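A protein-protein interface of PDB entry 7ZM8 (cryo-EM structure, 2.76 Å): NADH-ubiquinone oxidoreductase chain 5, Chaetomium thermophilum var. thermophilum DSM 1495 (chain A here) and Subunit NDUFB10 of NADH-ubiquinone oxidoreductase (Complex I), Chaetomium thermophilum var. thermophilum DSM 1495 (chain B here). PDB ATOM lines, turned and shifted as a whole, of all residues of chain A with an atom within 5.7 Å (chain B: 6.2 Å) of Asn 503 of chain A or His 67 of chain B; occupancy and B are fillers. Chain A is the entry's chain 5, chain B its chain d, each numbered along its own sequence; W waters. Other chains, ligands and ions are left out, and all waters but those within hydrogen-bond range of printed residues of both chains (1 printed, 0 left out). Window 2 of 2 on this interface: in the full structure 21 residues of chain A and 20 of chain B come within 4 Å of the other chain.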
ATOM      1  N   PHE A 198     -13.979  13.486   7.226  1.00  0.00           N
ATOM      2  CA  PHE A 198     -14.020  12.282   6.362  1.00  0.00           C
ATOM      3  C   PHE A 198     -15.322  12.240   5.559  1.00  0.00           C
ATOM      4  O   PHE A 198     -15.289  11.804   4.402  1.00  0.00           O
ATOM      5  CB  PHE A 198     -13.732  11.044   7.211  1.00  0.00           C
ATOM      6  CG  PHE A 198     -12.441  11.097   7.988  1.00  0.00           C
ATOM      7  CD1 PHE A 198     -11.360  11.831   7.528  1.00  0.00           C
ATOM      8  CD2 PHE A 198     -12.298  10.394   9.173  1.00  0.00           C
ATOM      9  CE1 PHE A 198     -10.178  11.886   8.248  1.00  0.00           C
ATOM     10  CE2 PHE A 198     -11.115  10.446   9.891  1.00  0.00           C
ATOM     11  CZ  PHE A 198     -10.058  11.192   9.427  1.00  0.00           C
ATOM     12  N   SER A 199     -16.422  12.714   6.137  1.00  0.00           N
ATOM     13  CA  SER A 199     -17.671  12.761   5.390  1.00  0.00           C
ATOM     14  C   SER A 199     -17.557  13.685   4.185  1.00  0.00           C
ATOM     15  O   SER A 199     -18.084  13.380   3.111  1.00  0.00           O
ATOM     16  CB  SER A 199     -18.808  13.204   6.306  1.00  0.00           C
ATOM     17  OG  SER A 199     -18.479  14.410   6.960  1.00  0.00           O
ATOM     18  N   PRO A 202     -14.458  13.469   0.032  1.00  0.00           N
ATOM     19  CA  PRO A 202     -14.520  13.192  -1.410  1.00  0.00           C
ATOM     20  C   PRO A 202     -14.790  14.410  -2.278  1.00  0.00           C
ATOM     21  O   PRO A 202     -14.561  14.344  -3.489  1.00  0.00           O
ATOM     22  CB  PRO A 202     -15.663  12.179  -1.515  1.00  0.00           C
ATOM     23  CG  PRO A 202     -15.714  11.554  -0.211  1.00  0.00           C
ATOM     24  CD  PRO A 202     -15.391  12.601   0.766  1.00  0.00           C
ATOM     25  N   SER A 264      -6.806   8.146   6.727  1.00  0.00           N
ATOM     26  CA  SER A 264      -7.048   7.420   5.485  1.00  0.00           C
ATOM     27  C   SER A 264      -8.280   7.892   4.712  1.00  0.00           C
ATOM     28  O   SER A 264      -8.194   7.965   3.475  1.00  0.00           O
ATOM     29  CB  SER A 264      -7.118   5.916   5.782  1.00  0.00           C
ATOM     30  OG  SER A 264      -8.196   5.589   6.631  1.00  0.00           O
ATOM     31  N   PRO A 265      -9.457   8.210   5.325  1.00  0.00           N
ATOM     32  CA  PRO A 265     -10.596   8.701   4.559  1.00  0.00           C
ATOM     33  C   PRO A 265     -10.364  10.059   3.888  1.00  0.00           C
ATOM     34  O   PRO A 265     -11.217  10.487   3.155  1.00  0.00           O
ATOM     35  CB  PRO A 265     -11.785   8.666   5.529  1.00  0.00           C
ATOM     36  CG  PRO A 265     -11.328   7.769   6.641  1.00  0.00           C
ATOM     37  CD  PRO A 265      -9.860   8.105   6.745  1.00  0.00           C
ATOM     38  N   PHE A 500     -12.705  -3.409   9.628  1.00  0.00           N
ATOM     39  CA  PHE A 500     -12.571  -1.959   9.580  1.00  0.00           C
ATOM     40  C   PHE A 500     -13.614  -1.344   8.657  1.00  0.00           C
ATOM     41  O   PHE A 500     -13.332  -0.408   7.909  1.00  0.00           O
ATOM     42  CB  PHE A 500     -11.157  -1.568   9.160  1.00  0.00           C
ATOM     43  CG  PHE A 500     -10.094  -2.235   9.971  1.00  0.00           C
ATOM     44  CD1 PHE A 500      -9.824  -1.816  11.258  1.00  0.00           C
ATOM     45  CD2 PHE A 500      -9.383  -3.301   9.462  1.00  0.00           C
ATOM     46  CE1 PHE A 500      -8.856  -2.438  12.017  1.00  0.00           C
ATOM     47  CE2 PHE A 500      -8.413  -3.923  10.215  1.00  0.00           C
ATOM     48  CZ  PHE A 500      -8.150  -3.491  11.495  1.00  0.00           C
ATOM     49  N   VAL A 501     -14.837  -1.867   8.718  1.00  0.00           N
ATOM     50  CA  VAL A 501     -15.900  -1.483   7.797  1.00  0.00           C
ATOM     51  C   VAL A 501     -16.755  -0.400   8.443  1.00  0.00           C
ATOM     52  O   VAL A 501     -17.810  -0.026   7.925  1.00  0.00           O
ATOM     53  CB  VAL A 501     -16.737  -2.709   7.390  1.00  0.00           C
ATOM     54  CG1 VAL A 501     -17.616  -3.160   8.525  1.00  0.00           C
ATOM     55  CG2 VAL A 501     -17.517  -2.455   6.119  1.00  0.00           C
ATOM     56  N   ASP A 502     -16.195   0.239   9.470  1.00  0.00           N
ATOM     57  CA  ASP A 502     -16.856   1.423  10.079  1.00  0.00           C
ATOM     58  C   ASP A 502     -16.078   2.645   9.577  1.00  0.00           C
ATOM     59  O   ASP A 502     -16.074   3.665  10.280  1.00  0.00           O
ATOM     60  CB  ASP A 502     -16.910   1.312  11.602  1.00  0.00           C
ATOM     61  CG  ASP A 502     -15.595   0.943  12.263  1.00  0.00           C
ATOM     62  OD1 ASP A 502     -14.943  -0.011  11.798  1.00  0.00           O
ATOM     63  OD2 ASP A 502     -15.238   1.610  13.245  1.00  0.00           O
ATOM     64  N   ASN A 503     -15.439   2.524   8.408  1.00  0.00           N
ATOM     65  CA  ASN A 503     -14.675   3.631   7.771  1.00  0.00           C
ATOM     66  C   ASN A 503     -13.515   4.072   8.666  1.00  0.00           C
ATOM     67  O   ASN A 503     -13.159   5.262   8.640  1.00  0.00           O
ATOM     68  CB  ASN A 503     -15.577   4.777   7.303  1.00  0.00           C
ATOM     69  CG  ASN A 503     -15.061   5.475   6.065  1.00  0.00           C
ATOM     70  OD1 ASN A 503     -14.795   6.673   6.087  1.00  0.00           O
ATOM     71  ND2 ASN A 503     -14.917   4.733   4.981  1.00  0.00           N
ATOM     72  N   SER A 504     -12.928   3.140   9.405  1.00  0.00           N
ATOM     73  CA  SER A 504     -11.741   3.510  10.209  1.00  0.00           C
ATOM     74  C   SER A 504     -10.533   3.429   9.282  1.00  0.00           C
ATOM     75  O   SER A 504      -9.600   4.227   9.466  1.00  0.00           O
ATOM     76  CB  SER A 504     -11.587   2.608  11.404  1.00  0.00           C
ATOM     77  OG  SER A 504     -12.777   2.580  12.174  1.00  0.00           O
ATOM     78  N   LEU A 505     -10.579   2.510   8.315  1.00  0.00           N
ATOM     79  CA  LEU A 505      -9.502   2.381   7.335  1.00  0.00           C
ATOM     80  C   LEU A 505     -10.140   2.328   5.954  1.00  0.00           C
ATOM     81  O   LEU A 505     -10.497   1.252   5.473  1.00  0.00           O
ATOM     82  CB  LEU A 505      -8.658   1.140   7.596  1.00  0.00           C
ATOM     83  CG  LEU A 505      -7.754   1.170   8.822  1.00  0.00           C
ATOM     84  CD1 LEU A 505      -6.941  -0.098   8.898  1.00  0.00           C
ATOM     85  CD2 LEU A 505      -6.861   2.386   8.789  1.00  0.00           C
ATOM     86  N   PHE A 506     -10.264   3.485   5.315  1.00  0.00           N
ATOM     87  CA  PHE A 506     -10.941   3.588   4.031  1.00  0.00           C
ATOM     88  C   PHE A 506      -9.950   3.365   2.896  1.00  0.00           C
ATOM     89  O   PHE A 506      -8.996   4.132   2.734  1.00  0.00           O
ATOM     90  CB  PHE A 506     -11.613   4.952   3.893  1.00  0.00           C
ATOM     91  CG  PHE A 506     -12.152   5.222   2.524  1.00  0.00           C
ATOM     92  CD1 PHE A 506     -13.080   4.373   1.952  1.00  0.00           C
ATOM     93  CD2 PHE A 506     -11.737   6.324   1.813  1.00  0.00           C
ATOM     94  CE1 PHE A 506     -13.576   4.619   0.702  1.00  0.00           C
ATOM     95  CE2 PHE A 506     -12.232   6.572   0.561  1.00  0.00           C
ATOM     96  CZ  PHE A 506     -13.155   5.719   0.006  1.00  0.00           C
ATOM     97  N   CYS B  59     -24.912  10.452  11.718  1.00  0.00           N
ATOM     98  CA  CYS B  59     -25.139   9.667  10.508  1.00  0.00           C
ATOM     99  C   CYS B  59     -23.854   8.986  10.064  1.00  0.00           C
ATOM    100  O   CYS B  59     -23.883   7.875   9.527  1.00  0.00           O
ATOM    101  CB  CYS B  59     -25.690  10.563   9.394  1.00  0.00           C
ATOM    102  SG  CYS B  59     -26.125   9.755   7.798  1.00  0.00           S
ATOM    103  N   TYR B  60     -22.711   9.627  10.296  1.00  0.00           N
ATOM    104  CA  TYR B  60     -21.402   9.034   9.913  1.00  0.00           C
ATOM    105  C   TYR B  60     -21.115   7.804  10.776  1.00  0.00           C
ATOM    106  O   TYR B  60     -20.712   6.770  10.224  1.00  0.00           O
ATOM    107  CB  TYR B  60     -20.277  10.056  10.079  1.00  0.00           C
ATOM    108  CG  TYR B  60     -18.913   9.572   9.657  1.00  0.00           C
ATOM    109  CD1 TYR B  60     -18.057   8.961  10.558  1.00  0.00           C
ATOM    110  CD2 TYR B  60     -18.477   9.726   8.353  1.00  0.00           C
ATOM    111  CE1 TYR B  60     -16.805   8.509  10.174  1.00  0.00           C
ATOM    112  CE2 TYR B  60     -17.230   9.284   7.954  1.00  0.00           C
ATOM    113  CZ  TYR B  60     -16.391   8.672   8.866  1.00  0.00           C
ATOM    114  OH  TYR B  60     -15.162   8.235   8.473  1.00  0.00           O
ATOM    115  N   GLU B  63     -23.758   4.962   9.879  1.00  0.00           N
ATOM    116  CA  GLU B  63     -23.691   4.308   8.581  1.00  0.00           C
ATOM    117  C   GLU B  63     -22.323   3.728   8.284  1.00  0.00           C
ATOM    118  O   GLU B  63     -22.218   2.802   7.475  1.00  0.00           O
ATOM    119  CB  GLU B  63     -24.082   5.294   7.476  1.00  0.00           C
ATOM    120  CG  GLU B  63     -25.476   5.906   7.591  1.00  0.00           C
ATOM    121  CD  GLU B  63     -26.563   4.962   8.095  1.00  0.00           C
ATOM    122  OE1 GLU B  63     -27.574   5.476   8.614  1.00  0.00           O
ATOM    123  OE2 GLU B  63     -26.468   3.731   7.907  1.00  0.00           O
ATOM    124  N   GLY B  64     -21.280   4.248   8.919  1.00  0.00           N
ATOM    125  CA  GLY B  64     -19.959   3.675   8.801  1.00  0.00           C
ATOM    126  C   GLY B  64     -19.410   3.663   7.393  1.00  0.00           C
ATOM    127  O   GLY B  64     -18.994   4.697   6.869  1.00  0.00           O
ATOM    128  N   VAL B  65     -19.383   2.481   6.781  1.00  0.00           N
ATOM    129  CA  VAL B  65     -18.788   2.348   5.458  1.00  0.00           C
ATOM    130  C   VAL B  65     -19.641   3.056   4.410  1.00  0.00           C
ATOM    131  O   VAL B  65     -19.128   3.821   3.585  1.00  0.00           O
ATOM    132  CB  VAL B  65     -18.565   0.863   5.117  1.00  0.00           C
ATOM    133  CG1 VAL B  65     -19.863   0.086   5.093  1.00  0.00           C
ATOM    134  CG2 VAL B  65     -17.820   0.721   3.836  1.00  0.00           C
ATOM    135  N   ASN B  66     -20.950   2.824   4.424  1.00  0.00           N
ATOM    136  CA  ASN B  66     -21.818   3.455   3.436  1.00  0.00           C
ATOM    137  C   ASN B  66     -22.447   4.733   3.970  1.00  0.00           C
ATOM    138  O   ASN B  66     -23.647   4.948   3.872  1.00  0.00           O
ATOM    139  CB  ASN B  66     -22.876   2.469   2.959  1.00  0.00           C
ATOM    140  CG  ASN B  66     -23.439   1.639   4.068  1.00  0.00           C
ATOM    141  OD1 ASN B  66     -23.775   2.153   5.129  1.00  0.00           O
ATOM    142  ND2 ASN B  66     -23.542   0.341   3.839  1.00  0.00           N
ATOM    143  N   HIS B  67     -21.597   5.653   4.394  1.00  0.00           N
ATOM    144  CA  HIS B  67     -22.064   7.004   4.767  1.00  0.00           C
ATOM    145  C   HIS B  67     -22.034   7.810   3.470  1.00  0.00           C
ATOM    146  O   HIS B  67     -22.734   8.819   3.385  1.00  0.00           O
ATOM    147  CB  HIS B  67     -21.089   7.603   5.790  1.00  0.00           C
ATOM    148  CG  HIS B  67     -19.746   7.941   5.237  1.00  0.00           C
ATOM    149  ND1 HIS B  67     -19.409   9.220   4.842  1.00  0.00           N
ATOM    150  CD2 HIS B  67     -18.659   7.178   5.001  1.00  0.00           C
ATOM    151  CE1 HIS B  67     -18.173   9.227   4.389  1.00  0.00           C
ATOM    152  NE2 HIS B  67     -17.695   7.989   4.474  1.00  0.00           N
ATOM    153  N   LEU B  68     -21.210   7.381   2.509  1.00  0.00           N
ATOM    154  CA  LEU B  68     -21.077   8.102   1.255  1.00  0.00           C
ATOM    155  C   LEU B  68     -22.331   8.027   0.397  1.00  0.00           C
ATOM    156  O   LEU B  68     -22.411   8.729  -0.614  1.00  0.00           O
ATOM    157  CB  LEU B  68     -19.877   7.560   0.488  1.00  0.00           C
ATOM    158  CG  LEU B  68     -18.553   8.222   0.864  1.00  0.00           C
ATOM    159  CD1 LEU B  68     -17.385   7.600   0.121  1.00  0.00           C
ATOM    160  CD2 LEU B  68     -18.636   9.707   0.614  1.00  0.00           C
ATOM    161  N   GLU B  69     -23.299   7.191   0.766  1.00  0.00           N
ATOM    162  CA  GLU B  69     -24.559   7.104   0.054  1.00  0.00           C
ATOM    163  C   GLU B  69     -25.767   7.226   0.965  1.00  0.00           C
ATOM    164  O   GLU B  69     -26.891   7.009   0.502  1.00  0.00           O
ATOM    165  CB  GLU B  69     -24.635   5.792  -0.737  1.00  0.00           C
ATOM    166  CG  GLU B  69     -24.517   4.540   0.094  1.00  0.00           C
ATOM    167  CD  GLU B  69     -25.859   3.942   0.458  1.00  0.00           C
ATOM    168  OE1 GLU B  69     -26.861   4.271  -0.210  1.00  0.00           O
ATOM    169  OE2 GLU B  69     -25.909   3.126   1.403  1.00  0.00           O
ATOM    170  N   LYS B  70     -25.575   7.567   2.237  1.00  0.00           N
ATOM    171  CA  LYS B  70     -26.671   7.714   3.177  1.00  0.00           C
ATOM    172  C   LYS B  70     -26.721   9.065   3.866  1.00  0.00           C
ATOM    173  O   LYS B  70     -27.752   9.387   4.466  1.00  0.00           O
ATOM    174  CB  LYS B  70     -26.600   6.621   4.254  1.00  0.00           C
ATOM    175  CG  LYS B  70     -26.717   5.213   3.726  1.00  0.00           C
ATOM    176  CD  LYS B  70     -28.050   4.989   3.052  1.00  0.00           C
ATOM    177  CE  LYS B  70     -29.183   5.049   4.061  1.00  0.00           C
ATOM    178  NZ  LYS B  70     -29.093   3.941   5.053  1.00  0.00           N
ATOM    179  N   CYS B  71     -25.653   9.858   3.805  1.00  0.00           N
ATOM    180  CA  CYS B  71     -25.561  11.106   4.550  1.00  0.00           C
ATOM    181  C   CYS B  71     -25.389  12.307   3.624  1.00  0.00           C
ATOM    182  O   CYS B  71     -24.832  13.327   4.024  1.00  0.00           O
ATOM    183  CB  CYS B  71     -24.420  11.041   5.568  1.00  0.00           C
ATOM    184  SG  CYS B  71     -24.422   9.615   6.690  1.00  0.00           S
ATOM    185  N   GLY B  72     -25.880  12.200   2.387  1.00  0.00           N
ATOM    186  CA  GLY B  72     -25.652  13.251   1.408  1.00  0.00           C
ATOM    187  C   GLY B  72     -26.482  14.499   1.613  1.00  0.00           C
ATOM    188  O   GLY B  72     -26.020  15.602   1.307  1.00  0.00           O
ATOM    189  N   ARG B  75     -24.808  16.495   4.195  1.00  0.00           N
ATOM    190  CA  ARG B  75     -23.598  17.065   3.616  1.00  0.00           C
ATOM    191  C   ARG B  75     -23.912  18.293   2.773  1.00  0.00           C
ATOM    192  O   ARG B  75     -23.176  19.284   2.812  1.00  0.00           O
ATOM    193  CB  ARG B  75     -22.877  16.015   2.778  1.00  0.00           C
ATOM    194  CG  ARG B  75     -21.998  15.086   3.571  1.00  0.00           C
ATOM    195  CD  ARG B  75     -21.120  14.303   2.653  1.00  0.00           C
ATOM    196  NE  ARG B  75     -21.880  13.667   1.585  1.00  0.00           N
ATOM    197  CZ  ARG B  75     -22.123  12.366   1.519  1.00  0.00           C
ATOM    198  NH1 ARG B  75     -22.815  11.874   0.508  1.00  0.00           N
ATOM    199  NH2 ARG B  75     -21.671  11.561   2.466  1.00  0.00           N
HETATM  200  O   HOH W   1     -13.264   7.220  10.437  1.00  0.00           O
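O of Val 501 of chain A sits close to N of Val 65 of chain B (3.2 Å). The side-chain amide oxygen (OD1) of Asn 503 of chain A sits at hydrogen-bond distance from the side-chain hydroxyl (OH) of Tyr 60 of chain B (2.9 Å).
O of His 67 of chain B sits at hydrogen-bond distance from NH2 of Arg 75 of chain B (3.1 Å). The guanidinium group of Arg 75 of chain B is in hydrogen-bond range of the backbone carbonyl oxygen of Leu 68 of chain B (3.4 Å). The side-chain sulfur (SG) of Cys 59 of chain B is disulfide-bonded to the side-chain sulfur (SG) of Cys 71 of chain B, at 2.0 Å.
Among the printed residues, merely in contact across the chains: Phe 198 of chain A with Tyr 60 of chain B (3.4 Å), Phe 198 of chain A with His 67 of chain B (3.9 Å), Ser 199 of chain A with Tyr 60 of chain B (3.96 Å), Ser 199 of chain A with His 67 of chain B (3.7 Å), Ser 199 of chain A with Arg 75 of chain B (3.2 Å), Pro 202 of chain A with Leu 68 of chain B (3.6 Å), Asn 503 of chain A with Gly 64 of chain B (3.4 Å) and Asn 503 of chain A with His 67 of chain B (3.6 Å).
Of chain B, only Tyr 60 (2.9 Å), Gly 64 (3.4 Å) and His 67 (3.6 Å) come within 4 Å of Asn 503 of chain A. His 67 of chain B touches three residues of chain A. Printed residues of chain B within 4 Å of Ser 199 of chain A: Tyr 60 (3.96 Å), His 67 (3.7 Å) and Arg 75 (3.2 Å). Printed residues of chain B within 4 Å of Val 501 of chain A: Val 65 (3.0 Å). The nearest printed residue of chain B that does not touch Phe 198 of chain A is Leu 68 of chain B (5.5 Å).
Of the 13 printed residues of chain B, 6 touch a printed residue of chain A. Printed residues of chain B that touch a printed residue of chain A: Tyr 60, Gly 64, Val 65, His 67, Leu 68 and Arg 75. Hydrophobic or aromatic side chains of chain B that line the printed part of chain A: Tyr 60, Val 65, His 67 and Leu 68. Along chain B the printed residues that touch a printed residue of chain A span positions 60 to 75. Of the 12 printed residues of chain A, 5 touch a printed residue of chain B. Among the printed residues, no Asp or Glu carboxylate lies within 4 Å of a Lys or Arg side-chain nitrogen of the other chain.
Water W1 lies within hydrogen-bond range of O of Asn 503 of chain A (2.7 Å) and OH of Tyr 60 of chain B (2.9 Å).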
